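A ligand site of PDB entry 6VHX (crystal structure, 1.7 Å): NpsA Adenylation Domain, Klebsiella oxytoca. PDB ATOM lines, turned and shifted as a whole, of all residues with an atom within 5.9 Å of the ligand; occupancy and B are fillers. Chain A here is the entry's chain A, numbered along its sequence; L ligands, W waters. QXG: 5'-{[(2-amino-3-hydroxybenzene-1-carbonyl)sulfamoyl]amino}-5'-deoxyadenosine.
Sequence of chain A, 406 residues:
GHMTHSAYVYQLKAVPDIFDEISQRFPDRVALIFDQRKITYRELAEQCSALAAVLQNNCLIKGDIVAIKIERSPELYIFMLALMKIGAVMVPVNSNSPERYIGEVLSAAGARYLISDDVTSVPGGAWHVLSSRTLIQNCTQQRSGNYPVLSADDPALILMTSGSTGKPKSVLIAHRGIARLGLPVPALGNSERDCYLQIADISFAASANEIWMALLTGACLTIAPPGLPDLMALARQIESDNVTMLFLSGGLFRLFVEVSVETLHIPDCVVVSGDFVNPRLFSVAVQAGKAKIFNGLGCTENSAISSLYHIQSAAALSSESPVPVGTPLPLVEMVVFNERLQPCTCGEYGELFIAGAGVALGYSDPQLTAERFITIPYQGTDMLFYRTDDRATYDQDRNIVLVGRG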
ATOM      1  N   THR A 161      15.946  13.427   1.815  1.00  0.00           N
ATOM      2  CA  THR A 161      14.621  12.923   1.481  1.00  0.00           C
ATOM      3  C   THR A 161      14.678  12.189   0.150  1.00  0.00           C
ATOM      4  O   THR A 161      15.734  12.061  -0.466  1.00  0.00           O
ATOM      5  CB  THR A 161      13.576  14.045   1.454  1.00  0.00           C
ATOM      6  OG1 THR A 161      12.261  13.479   1.550  1.00  0.00           O
ATOM      7  CG2 THR A 161      13.680  14.861   0.182  1.00  0.00           C
ATOM      8  N   SER A 162      13.519  11.682  -0.288  1.00  0.00           N
ATOM      9  CA  SER A 162      13.399  11.019  -1.575  1.00  0.00           C
ATOM     10  C   SER A 162      12.153  11.513  -2.280  1.00  0.00           C
ATOM     11  O   SER A 162      11.138  11.820  -1.651  1.00  0.00           O
ATOM     12  CB  SER A 162      13.315   9.489  -1.442  1.00  0.00           C
ATOM     13  OG  SER A 162      14.488   8.971  -0.838  1.00  0.00           O
ATOM     14  N   PHE A 204      14.733  12.912  10.441  1.00  0.00           N
ATOM     15  CA  PHE A 204      13.456  13.019   9.751  1.00  0.00           C
ATOM     16  C   PHE A 204      12.855  14.373  10.132  1.00  0.00           C
ATOM     17  O   PHE A 204      12.908  14.778  11.293  1.00  0.00           O
ATOM     18  CB  PHE A 204      12.544  11.857  10.198  1.00  0.00           C
ATOM     19  CG  PHE A 204      11.218  11.809   9.515  1.00  0.00           C
ATOM     20  CD1 PHE A 204      10.986  12.466   8.322  1.00  0.00           C
ATOM     21  CD2 PHE A 204      10.172  11.085  10.085  1.00  0.00           C
ATOM     22  CE1 PHE A 204       9.748  12.426   7.718  1.00  0.00           C
ATOM     23  CE2 PHE A 204       8.920  11.016   9.481  1.00  0.00           C
ATOM     24  CZ  PHE A 204       8.713  11.693   8.288  1.00  0.00           C
ATOM     25  N   ALA A 205      12.320  15.085   9.127  1.00  0.00           N
ATOM     26  CA  ALA A 205      11.729  16.396   9.390  1.00  0.00           C
ATOM     27  C   ALA A 205      10.623  16.336  10.425  1.00  0.00           C
ATOM     28  O   ALA A 205      10.407  17.314  11.155  1.00  0.00           O
ATOM     29  CB  ALA A 205      11.193  16.996   8.086  1.00  0.00           C
ATOM     30  N   ALA A 206       9.901  15.230  10.506  1.00  0.00           N
ATOM     31  CA  ALA A 206       8.846  15.122  11.513  1.00  0.00           C
ATOM     32  C   ALA A 206       9.352  15.334  12.938  1.00  0.00           C
ATOM     33  O   ALA A 206       8.549  15.726  13.796  1.00  0.00           O
ATOM     34  CB  ALA A 206       8.148  13.773  11.402  1.00  0.00           C
ATOM     35  N   SER A 207      10.630  15.096  13.230  1.00  0.00           N
ATOM     36  CA  SER A 207      11.116  15.342  14.587  1.00  0.00           C
ATOM     37  C   SER A 207      10.999  16.812  14.960  1.00  0.00           C
ATOM     38  O   SER A 207      10.871  17.145  16.147  1.00  0.00           O
ATOM     39  CB  SER A 207      12.577  14.870  14.740  1.00  0.00           C
ATOM     40  OG  SER A 207      13.479  15.585  13.895  1.00  0.00           O
ATOM     41  N   ASN A 209       8.511  18.734  14.530  1.00  0.00           N
ATOM     42  CA  ASN A 209       7.203  18.929  15.158  1.00  0.00           C
ATOM     43  C   ASN A 209       7.315  18.793  16.661  1.00  0.00           C
ATOM     44  O   ASN A 209       6.731  19.573  17.424  1.00  0.00           O
ATOM     45  CB  ASN A 209       6.168  17.902  14.685  1.00  0.00           C
ATOM     46  CG  ASN A 209       6.080  17.734  13.181  1.00  0.00           C
ATOM     47  OD1 ASN A 209       6.543  18.576  12.409  1.00  0.00           O
ATOM     48  ND2 ASN A 209       5.451  16.640  12.752  1.00  0.00           N
ATOM     49  N   PHE A 247       2.508  13.459  18.499  1.00  0.00           N
ATOM     50  CA  PHE A 247       2.714  13.301  17.051  1.00  0.00           C
ATOM     51  C   PHE A 247       3.114  11.859  16.768  1.00  0.00           C
ATOM     52  O   PHE A 247       4.012  11.332  17.416  1.00  0.00           O
ATOM     53  CB  PHE A 247       3.820  14.252  16.526  1.00  0.00           C
ATOM     54  CG  PHE A 247       3.389  15.682  16.423  1.00  0.00           C
ATOM     55  CD1 PHE A 247       3.580  16.557  17.473  1.00  0.00           C
ATOM     56  CD2 PHE A 247       2.783  16.156  15.261  1.00  0.00           C
ATOM     57  CE1 PHE A 247       3.172  17.880  17.372  1.00  0.00           C
ATOM     58  CE2 PHE A 247       2.383  17.454  15.142  1.00  0.00           C
ATOM     59  CZ  PHE A 247       2.568  18.322  16.194  1.00  0.00           C
ATOM     60  N   VAL A 272      -1.414  12.462  13.215  1.00  0.00           N
ATOM     61  CA  VAL A 272      -0.857  11.371  12.424  1.00  0.00           C
ATOM     62  C   VAL A 272      -0.398  11.962  11.102  1.00  0.00           C
ATOM     63  O   VAL A 272      -1.207  12.536  10.360  1.00  0.00           O
ATOM     64  CB  VAL A 272      -1.897  10.264  12.198  1.00  0.00           C
ATOM     65  CG1 VAL A 272      -1.220   9.047  11.557  1.00  0.00           C
ATOM     66  CG2 VAL A 272      -2.549   9.873  13.521  1.00  0.00           C
ATOM     67  N   SER A 273       0.879  11.815  10.775  1.00  0.00           N
ATOM     68  CA  SER A 273       1.364  12.370   9.528  1.00  0.00           C
ATOM     69  C   SER A 273       2.305  11.404   8.846  1.00  0.00           C
ATOM     70  O   SER A 273       2.825  10.459   9.465  1.00  0.00           O
ATOM     71  CB  SER A 273       2.058  13.724   9.734  1.00  0.00           C
ATOM     72  OG  SER A 273       3.299  13.581  10.428  1.00  0.00           O
ATOM     73  N   GLY A 274       2.519  11.621   7.547  1.00  0.00           N
ATOM     74  CA  GLY A 274       3.586  10.932   6.855  1.00  0.00           C
ATOM     75  C   GLY A 274       3.152  10.198   5.606  1.00  0.00           C
ATOM     76  O   GLY A 274       3.958  10.031   4.686  1.00  0.00           O
ATOM     77  N   ASP A 275       1.899   9.771   5.545  1.00  0.00           N
ATOM     78  CA  ASP A 275       1.452   8.913   4.459  1.00  0.00           C
ATOM     79  C   ASP A 275      -0.052   8.714   4.599  1.00  0.00           C
ATOM     80  O   ASP A 275      -0.661   9.134   5.575  1.00  0.00           O
ATOM     81  CB  ASP A 275       2.215   7.588   4.507  1.00  0.00           C
ATOM     82  CG  ASP A 275       1.982   6.708   3.290  1.00  0.00           C
ATOM     83  OD1 ASP A 275       1.393   7.177   2.286  1.00  0.00           O
ATOM     84  OD2 ASP A 275       2.388   5.523   3.367  1.00  0.00           O
ATOM     85  N   PHE A 276      -0.644   8.094   3.586  1.00  0.00           N
ATOM     86  CA  PHE A 276      -2.063   7.751   3.681  1.00  0.00           C
ATOM     87  C   PHE A 276      -2.264   6.744   4.798  1.00  0.00           C
ATOM     88  O   PHE A 276      -1.432   5.852   5.005  1.00  0.00           O
ATOM     89  CB  PHE A 276      -2.584   7.193   2.363  1.00  0.00           C
ATOM     90  CG  PHE A 276      -2.620   8.205   1.259  1.00  0.00           C
ATOM     91  CD1 PHE A 276      -3.619   9.156   1.212  1.00  0.00           C
ATOM     92  CD2 PHE A 276      -1.631   8.229   0.277  1.00  0.00           C
ATOM     93  CE1 PHE A 276      -3.648  10.095   0.185  1.00  0.00           C
ATOM     94  CE2 PHE A 276      -1.653   9.164  -0.743  1.00  0.00           C
ATOM     95  CZ  PHE A 276      -2.664  10.100  -0.786  1.00  0.00           C
ATOM     96  N   VAL A 277      -3.370   6.887   5.514  1.00  0.00           N
ATOM     97  CA  VAL A 277      -3.741   5.973   6.590  1.00  0.00           C
ATOM     98  C   VAL A 277      -5.105   5.408   6.251  1.00  0.00           C
ATOM     99  O   VAL A 277      -6.001   6.153   5.862  1.00  0.00           O
ATOM    100  CB  VAL A 277      -3.782   6.693   7.957  1.00  0.00           C
ATOM    101  CG1 VAL A 277      -4.288   5.745   9.045  1.00  0.00           C
ATOM    102  CG2 VAL A 277      -2.412   7.231   8.307  1.00  0.00           C
ATOM    103  N   ASN A 295      -5.418  14.135  10.931  1.00  0.00           N
ATOM    104  CA  ASN A 295      -4.596  13.750   9.793  1.00  0.00           C
ATOM    105  C   ASN A 295      -3.746  14.968   9.418  1.00  0.00           C
ATOM    106  O   ASN A 295      -4.299  16.048   9.172  1.00  0.00           O
ATOM    107  CB  ASN A 295      -5.464  13.307   8.617  1.00  0.00           C
ATOM    108  CG  ASN A 295      -4.661  12.725   7.466  1.00  0.00           C
ATOM    109  OD1 ASN A 295      -3.572  12.163   7.662  1.00  0.00           O
ATOM    110  ND2 ASN A 295      -5.194  12.855   6.252  1.00  0.00           N
ATOM    111  N   GLY A 296      -2.440  14.795   9.389  1.00  0.00           N
ATOM    112  CA  GLY A 296      -1.512  15.904   9.153  1.00  0.00           C
ATOM    113  C   GLY A 296      -0.628  15.646   7.954  1.00  0.00           C
ATOM    114  O   GLY A 296      -0.212  14.513   7.708  1.00  0.00           O
ATOM    115  N   LEU A 297      -0.376  16.700   7.176  1.00  0.00           N
ATOM    116  CA  LEU A 297       0.567  16.621   6.074  1.00  0.00           C
ATOM    117  C   LEU A 297       1.841  17.357   6.447  1.00  0.00           C
ATOM    118  O   LEU A 297       1.794  18.488   6.950  1.00  0.00           O
ATOM    119  CB  LEU A 297       0.000  17.238   4.794  1.00  0.00           C
ATOM    120  CG  LEU A 297       1.059  17.366   3.688  1.00  0.00           C
ATOM    121  CD1 LEU A 297       1.213  16.065   2.931  1.00  0.00           C
ATOM    122  CD2 LEU A 297       0.734  18.521   2.755  1.00  0.00           C
ATOM    123  N   GLY A 298       2.976  16.713   6.223  1.00  0.00           N
ATOM    124  CA  GLY A 298       4.251  17.398   6.293  1.00  0.00           C
ATOM    125  C   GLY A 298       5.099  16.955   5.117  1.00  0.00           C
ATOM    126  O   GLY A 298       4.870  15.896   4.535  1.00  0.00           O
ATOM    127  N   CYS A 299       6.103  17.771   4.791  1.00  0.00           N
ATOM    128  CA  CYS A 299       7.114  17.268   3.885  1.00  0.00           C
ATOM    129  C   CYS A 299       8.414  17.981   4.207  1.00  0.00           C
ATOM    130  O   CYS A 299       8.415  19.080   4.767  1.00  0.00           O
ATOM    131  CB  CYS A 299       6.746  17.442   2.414  1.00  0.00           C
ATOM    132  SG  CYS A 299       6.613  19.137   1.878  1.00  0.00           S
ATOM    133  N   THR A 300       9.517  17.274   3.897  1.00  0.00           N
ATOM    134  CA  THR A 300      10.843  17.755   4.250  1.00  0.00           C
ATOM    135  C   THR A 300      11.081  19.157   3.688  1.00  0.00           C
ATOM    136  O   THR A 300      11.620  20.036   4.387  1.00  0.00           O
ATOM    137  CB  THR A 300      11.900  16.773   3.727  1.00  0.00           C
ATOM    138  OG1 THR A 300      11.663  15.476   4.292  1.00  0.00           O
ATOM    139  CG2 THR A 300      13.289  17.219   4.120  1.00  0.00           C
ATOM    140  N   GLU A 301      10.638  19.392   2.450  1.00  0.00           N
ATOM    141  CA  GLU A 301      10.836  20.663   1.779  1.00  0.00           C
ATOM    142  C   GLU A 301      10.005  21.798   2.357  1.00  0.00           C
ATOM    143  O   GLU A 301      10.180  22.942   1.945  1.00  0.00           O
ATOM    144  CB  GLU A 301      10.540  20.504   0.291  1.00  0.00           C
ATOM    145  CG  GLU A 301      11.538  19.634  -0.446  1.00  0.00           C
ATOM    146  CD  GLU A 301      11.154  18.181  -0.485  1.00  0.00           C
ATOM    147  OE1 GLU A 301      10.353  17.722   0.350  1.00  0.00           O
ATOM    148  OE2 GLU A 301      11.671  17.479  -1.382  1.00  0.00           O
ATOM    149  N   SER A 303       9.883  21.820   5.893  1.00  0.00           N
ATOM    150  CA  SER A 303      10.598  21.866   7.171  1.00  0.00           C
ATOM    151  C   SER A 303       9.938  21.076   8.305  1.00  0.00           C
ATOM    152  O   SER A 303      10.646  20.600   9.205  1.00  0.00           O
ATOM    153  CB  SER A 303      10.793  23.311   7.654  1.00  0.00           C
ATOM    154  OG  SER A 303      11.406  24.108   6.642  1.00  0.00           O
ATOM    155  N   ALA A 304       8.608  20.988   8.312  1.00  0.00           N
ATOM    156  CA  ALA A 304       7.884  20.415   9.446  1.00  0.00           C
ATOM    157  C   ALA A 304       6.408  20.261   9.065  1.00  0.00           C
ATOM    158  O   ALA A 304       6.002  20.552   7.935  1.00  0.00           O
ATOM    159  CB  ALA A 304       8.028  21.294  10.691  1.00  0.00           C
ATOM    160  N   ILE A 305       5.610  19.814  10.035  1.00  0.00           N
ATOM    161  CA  ILE A 305       4.173  19.637   9.812  1.00  0.00           C
ATOM    162  C   ILE A 305       3.588  20.925   9.221  1.00  0.00           C
ATOM    163  O   ILE A 305       4.001  22.039   9.592  1.00  0.00           O
ATOM    164  CB  ILE A 305       3.497  19.251  11.131  1.00  0.00           C
ATOM    165  CG1 ILE A 305       2.009  18.892  10.905  1.00  0.00           C
ATOM    166  CG2 ILE A 305       3.708  20.347  12.189  1.00  0.00           C
ATOM    167  CD1 ILE A 305       1.821  17.578  10.136  1.00  0.00           C
ATOM    168  N   SER A 306       2.647  20.766   8.288  1.00  0.00           N
ATOM    169  CA  SER A 306       2.250  21.840   7.373  1.00  0.00           C
ATOM    170  C   SER A 306       0.737  22.081   7.313  1.00  0.00           C
ATOM    171  O   SER A 306       0.298  23.216   7.068  1.00  0.00           O
ATOM    172  CB  SER A 306       2.806  21.519   5.981  1.00  0.00           C
ATOM    173  OG  SER A 306       4.240  21.475   6.018  1.00  0.00           O
ATOM    174  N   VAL A 325      -6.227  16.393   4.203  1.00  0.00           N
ATOM    175  CA  VAL A 325      -5.137  16.909   5.021  1.00  0.00           C
ATOM    176  C   VAL A 325      -5.421  18.300   5.564  1.00  0.00           C
ATOM    177  O   VAL A 325      -4.577  18.857   6.274  1.00  0.00           O
ATOM    178  CB  VAL A 325      -3.798  16.895   4.254  1.00  0.00           C
ATOM    179  CG1 VAL A 325      -3.342  15.445   4.000  1.00  0.00           C
ATOM    180  CG2 VAL A 325      -3.923  17.657   2.946  1.00  0.00           C
ATOM    181  N   TYR A 386       6.893  25.462  -3.162  1.00  0.00           N
ATOM    182  CA  TYR A 386       7.438  24.126  -3.362  1.00  0.00           C
ATOM    183  C   TYR A 386       6.389  23.257  -4.043  1.00  0.00           C
ATOM    184  O   TYR A 386       5.228  23.217  -3.606  1.00  0.00           O
ATOM    185  CB  TYR A 386       7.862  23.495  -2.021  1.00  0.00           C
ATOM    186  CG  TYR A 386       8.100  22.016  -2.150  1.00  0.00           C
ATOM    187  CD1 TYR A 386       9.126  21.541  -2.969  1.00  0.00           C
ATOM    188  CD2 TYR A 386       7.289  21.085  -1.491  1.00  0.00           C
ATOM    189  CE1 TYR A 386       9.325  20.184  -3.135  1.00  0.00           C
ATOM    190  CE2 TYR A 386       7.508  19.719  -1.637  1.00  0.00           C
ATOM    191  CZ  TYR A 386       8.529  19.285  -2.462  1.00  0.00           C
ATOM    192  OH  TYR A 386       8.741  17.933  -2.624  1.00  0.00           O
ATOM    193  N   THR A 388       4.897  19.762  -4.669  1.00  0.00           N
ATOM    194  CA  THR A 388       4.975  18.544  -3.846  1.00  0.00           C
ATOM    195  C   THR A 388       4.995  17.256  -4.644  1.00  0.00           C
ATOM    196  O   THR A 388       5.311  16.211  -4.063  1.00  0.00           O
ATOM    197  CB  THR A 388       3.784  18.422  -2.889  1.00  0.00           C
ATOM    198  OG1 THR A 388       2.569  18.357  -3.645  1.00  0.00           O
ATOM    199  CG2 THR A 388       3.736  19.578  -1.904  1.00  0.00           C
ATOM    200  N   ASP A 390       2.418  15.800  -5.192  1.00  0.00           N
ATOM    201  CA  ASP A 390       1.246  15.131  -4.634  1.00  0.00           C
ATOM    202  C   ASP A 390      -0.012  15.564  -5.399  1.00  0.00           C
ATOM    203  O   ASP A 390      -0.342  16.756  -5.431  1.00  0.00           O
ATOM    204  CB  ASP A 390       1.089  15.468  -3.153  1.00  0.00           C
ATOM    205  CG  ASP A 390       2.186  14.872  -2.305  1.00  0.00           C
ATOM    206  OD1 ASP A 390       2.408  13.648  -2.404  1.00  0.00           O
ATOM    207  OD2 ASP A 390       2.821  15.620  -1.540  1.00  0.00           O
ATOM    208  N   LEU A 402      -5.306  14.940  -0.514  1.00  0.00           N
ATOM    209  CA  LEU A 402      -4.396  14.237  -1.398  1.00  0.00           C
ATOM    210  C   LEU A 402      -5.072  12.981  -1.929  1.00  0.00           C
ATOM    211  O   LEU A 402      -5.801  12.294  -1.195  1.00  0.00           O
ATOM    212  CB  LEU A 402      -3.110  13.875  -0.672  1.00  0.00           C
ATOM    213  CG  LEU A 402      -2.321  15.008  -0.042  1.00  0.00           C
ATOM    214  CD1 LEU A 402      -0.912  14.535   0.323  1.00  0.00           C
ATOM    215  CD2 LEU A 402      -2.260  16.211  -0.948  1.00  0.00           C
HETATM  216  N10 QXG L   1       2.609  12.452   2.993  1.00  0.00           N
HETATM  217  C02 QXG L   1      -0.559  12.524   4.716  1.00  0.00           C
HETATM  218  C04 QXG L   1      -0.881  11.453   2.617  1.00  0.00           C
HETATM  219  C06 QXG L   1       1.236  12.167   3.099  1.00  0.00           C
HETATM  220  C07 QXG L   1       0.832  12.697   4.366  1.00  0.00           C
HETATM  221  C09 QXG L   1       2.995  13.114   4.181  1.00  0.00           C
HETATM  222  C11 QXG L   1       3.394  12.087   1.871  1.00  0.00           C
HETATM  223  C13 QXG L   1       5.443  13.122   1.463  1.00  0.00           C
HETATM  224  C14 QXG L   1       6.551  13.811   2.255  1.00  0.00           C
HETATM  225  C20 QXG L   1       7.258  13.918   6.050  1.00  0.00           C
HETATM  226  C22 QXG L   1       7.047  14.931   7.172  1.00  0.00           C
HETATM  227  C23 QXG L   1       7.780  16.142   7.129  1.00  0.00           C
HETATM  228  C24 QXG L   1       7.633  17.112   8.140  1.00  0.00           C
HETATM  229  C25 QXG L   1       6.758  16.843   9.207  1.00  0.00           C
HETATM  230  C26 QXG L   1       6.016  15.653   9.255  1.00  0.00           C
HETATM  231  C28 QXG L   1       6.164  14.638   8.223  1.00  0.00           C
HETATM  232  C30 QXG L   1       4.364  14.105   0.965  1.00  0.00           C
HETATM  233  C32 QXG L   1       3.208  13.091   0.704  1.00  0.00           C
HETATM  234  N01 QXG L   1      -1.103  12.990   5.928  1.00  0.00           N
HETATM  235  N03 QXG L   1      -1.391  11.917   3.825  1.00  0.00           N
HETATM  236  N05 QXG L   1       0.411  11.546   2.180  1.00  0.00           N
HETATM  237  N08 QXG L   1       1.931  13.261   5.021  1.00  0.00           N
HETATM  238  N15 QXG L   1       7.354  12.940   3.029  1.00  0.00           N
HETATM  239  N19 QXG L   1       8.275  14.288   5.126  1.00  0.00           N
HETATM  240  N29 QXG L   1       5.433  13.439   8.314  1.00  0.00           N
HETATM  241  O12 QXG L   1       4.800  12.276   2.365  1.00  0.00           O
HETATM  242  O17 QXG L   1       9.396  12.239   4.319  1.00  0.00           O
HETATM  243  O18 QXG L   1       9.488  14.193   2.962  1.00  0.00           O
HETATM  244  O21 QXG L   1       6.663  12.933   5.902  1.00  0.00           O
HETATM  245  O27 QXG L   1       5.192  15.437  10.283  1.00  0.00           O
HETATM  246  O31 QXG L   1       4.724  14.774  -0.225  1.00  0.00           O
HETATM  247  O33 QXG L   1       3.571  12.368  -0.493  1.00  0.00           O
HETATM  248  S16 QXG L   1       8.689  13.402   3.863  1.00  0.00           S
HETATM  249  O   HOH W   1       6.676  10.500   4.721  1.00  0.00           O
HETATM  250  O   HOH W   2      -4.071  11.771   3.886  1.00  0.00           O
HETATM  251  O   HOH W   3       9.603  15.194   0.413  1.00  0.00           O
HETATM  252  O   HOH W   4       5.483  11.247  10.687  1.00  0.00           O
HETATM  253  O   HOH W   5       8.691   8.827   4.183  1.00  0.00           O
HETATM  254  O   HOH W   6       6.988  16.280  -1.112  1.00  0.00           O
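ND2 of Asn 209 lies within hydrogen-bond range of O27 of the ligand, 2.8 Å away. OD1 of Asn 295 lies within hydrogen-bond range of N01 of the ligand, 3.1 Å away. The side-chain hydroxyl (OG1) of Thr 300 sits at hydrogen-bond distance from an oxygen (O18) of the ligand, at 2.9 Å. An oxygen (O18) of the ligand is in hydrogen-bond range of the backbone NH (N) of Thr 300. The backbone carbonyl oxygen (O) of Gly 296 lies within hydrogen-bond range of a nitrogen (N01) of the ligand. The backbone NH (N) of Gly 274 sits at hydrogen-bond distance from a nitrogen (N08) of the ligand (3.1 Å). The side-chain hydroxyl (OG1) of Thr 161 is in hydrogen-bond range of an oxygen (O18) of the ligand (3.2 Å). An oxygen (O31) of the ligand sits at hydrogen-bond distance from the side-chain carboxylate (OD2) of Asp 390 (2.5 Å). OG of Ser 273 lies within hydrogen-bond range of O27 of the ligand, at 2.7 Å.
The backbone carbonyl oxygen of Ala 206 lies close to the side-chain amide nitrogen of Asn 209 (3.4 Å). The side-chain hydroxyl of Thr 388 sits at hydrogen-bond distance from the backbone NH of Asp 390 (3.0 Å). The side-chain hydroxyl (OG) of Ser 207 sits at hydrogen-bond distance from the backbone carbonyl oxygen (O) of Phe 204, at 2.8 Å. The side-chain hydroxyl (OG1) of Thr 161 is in hydrogen-bond range of the side-chain hydroxyl (OG1) of Thr 300 (3.4 Å). N of Gly 296 sits at hydrogen-bond distance from O of Val 272, 2.8 Å away. O of Ala 304 is in hydrogen-bond range of OG of Ser 306, at 2.8 Å. The side-chain amide oxygen (OD1) of Asn 209 sits at hydrogen-bond distance from the backbone NH (N) of Ile 305 (2.8 Å). O of Leu 297 lies within hydrogen-bond range of N of Ser 306, at 2.8 Å.
The backbone carbonyl oxygen of Asp 275 sits close to a nitrogen (N03) of the ligand, at 3.4 Å. Merely in contact with the ligand: Ile 305 (3.3 Å), Cys 299 (3.3 Å), Phe 204 (3.3 Å), Gly 298 (3.4 Å), Ala 304 (3.4 Å), Phe 276 (3.5 Å), Ala 206 (3.6 Å), Ala 205 (3.6 Å), Leu 297 (3.6 Å), Leu 402 (3.8 Å) and Val 325 (3.8 Å). Hydrophobic or aromatic side chains that line the ligand: Phe 204, Ala 205, Ala 206, Phe 276, Leu 297, Ile 305, Val 325 and Leu 402. Within 4 Å of the ligand: Thr 161, Phe 204, Ala 205, Ala 206, Asn 209, Ser 273, Gly 274, Asp 275, Phe 276, Asn 295, Gly 296, Leu 297, Gly 298, Cys 299, Thr 300, Ala 304, Ile 305, Val 325, Asp 390 and Leu 402. The nearest printed residue that does not touch the ligand is Thr 388 (4.1 Å).
Water W2 bridges N03 of the ligand and ND2 of Asn 295. Water W1 bridges an oxygen (O21) of the ligand and the backbone carbonyl oxygen (O) of Gly 274. Water W3 lies within hydrogen-bond range of the side-chain carboxylate (OE1) of Glu 301 (2.6 Å), an oxygen (O18) of the ligand (2.7 Å) and the side-chain hydroxyl (OG1) of Thr 161 (3.4 Å). Water W6 lies within hydrogen-bond range of OH of Tyr 386, O31 of the ligand and O of Thr 388. Water W4 lies within hydrogen-bond range of O of Ser 273 (3.0 Å) and N29 of the ligand (3.2 Å).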
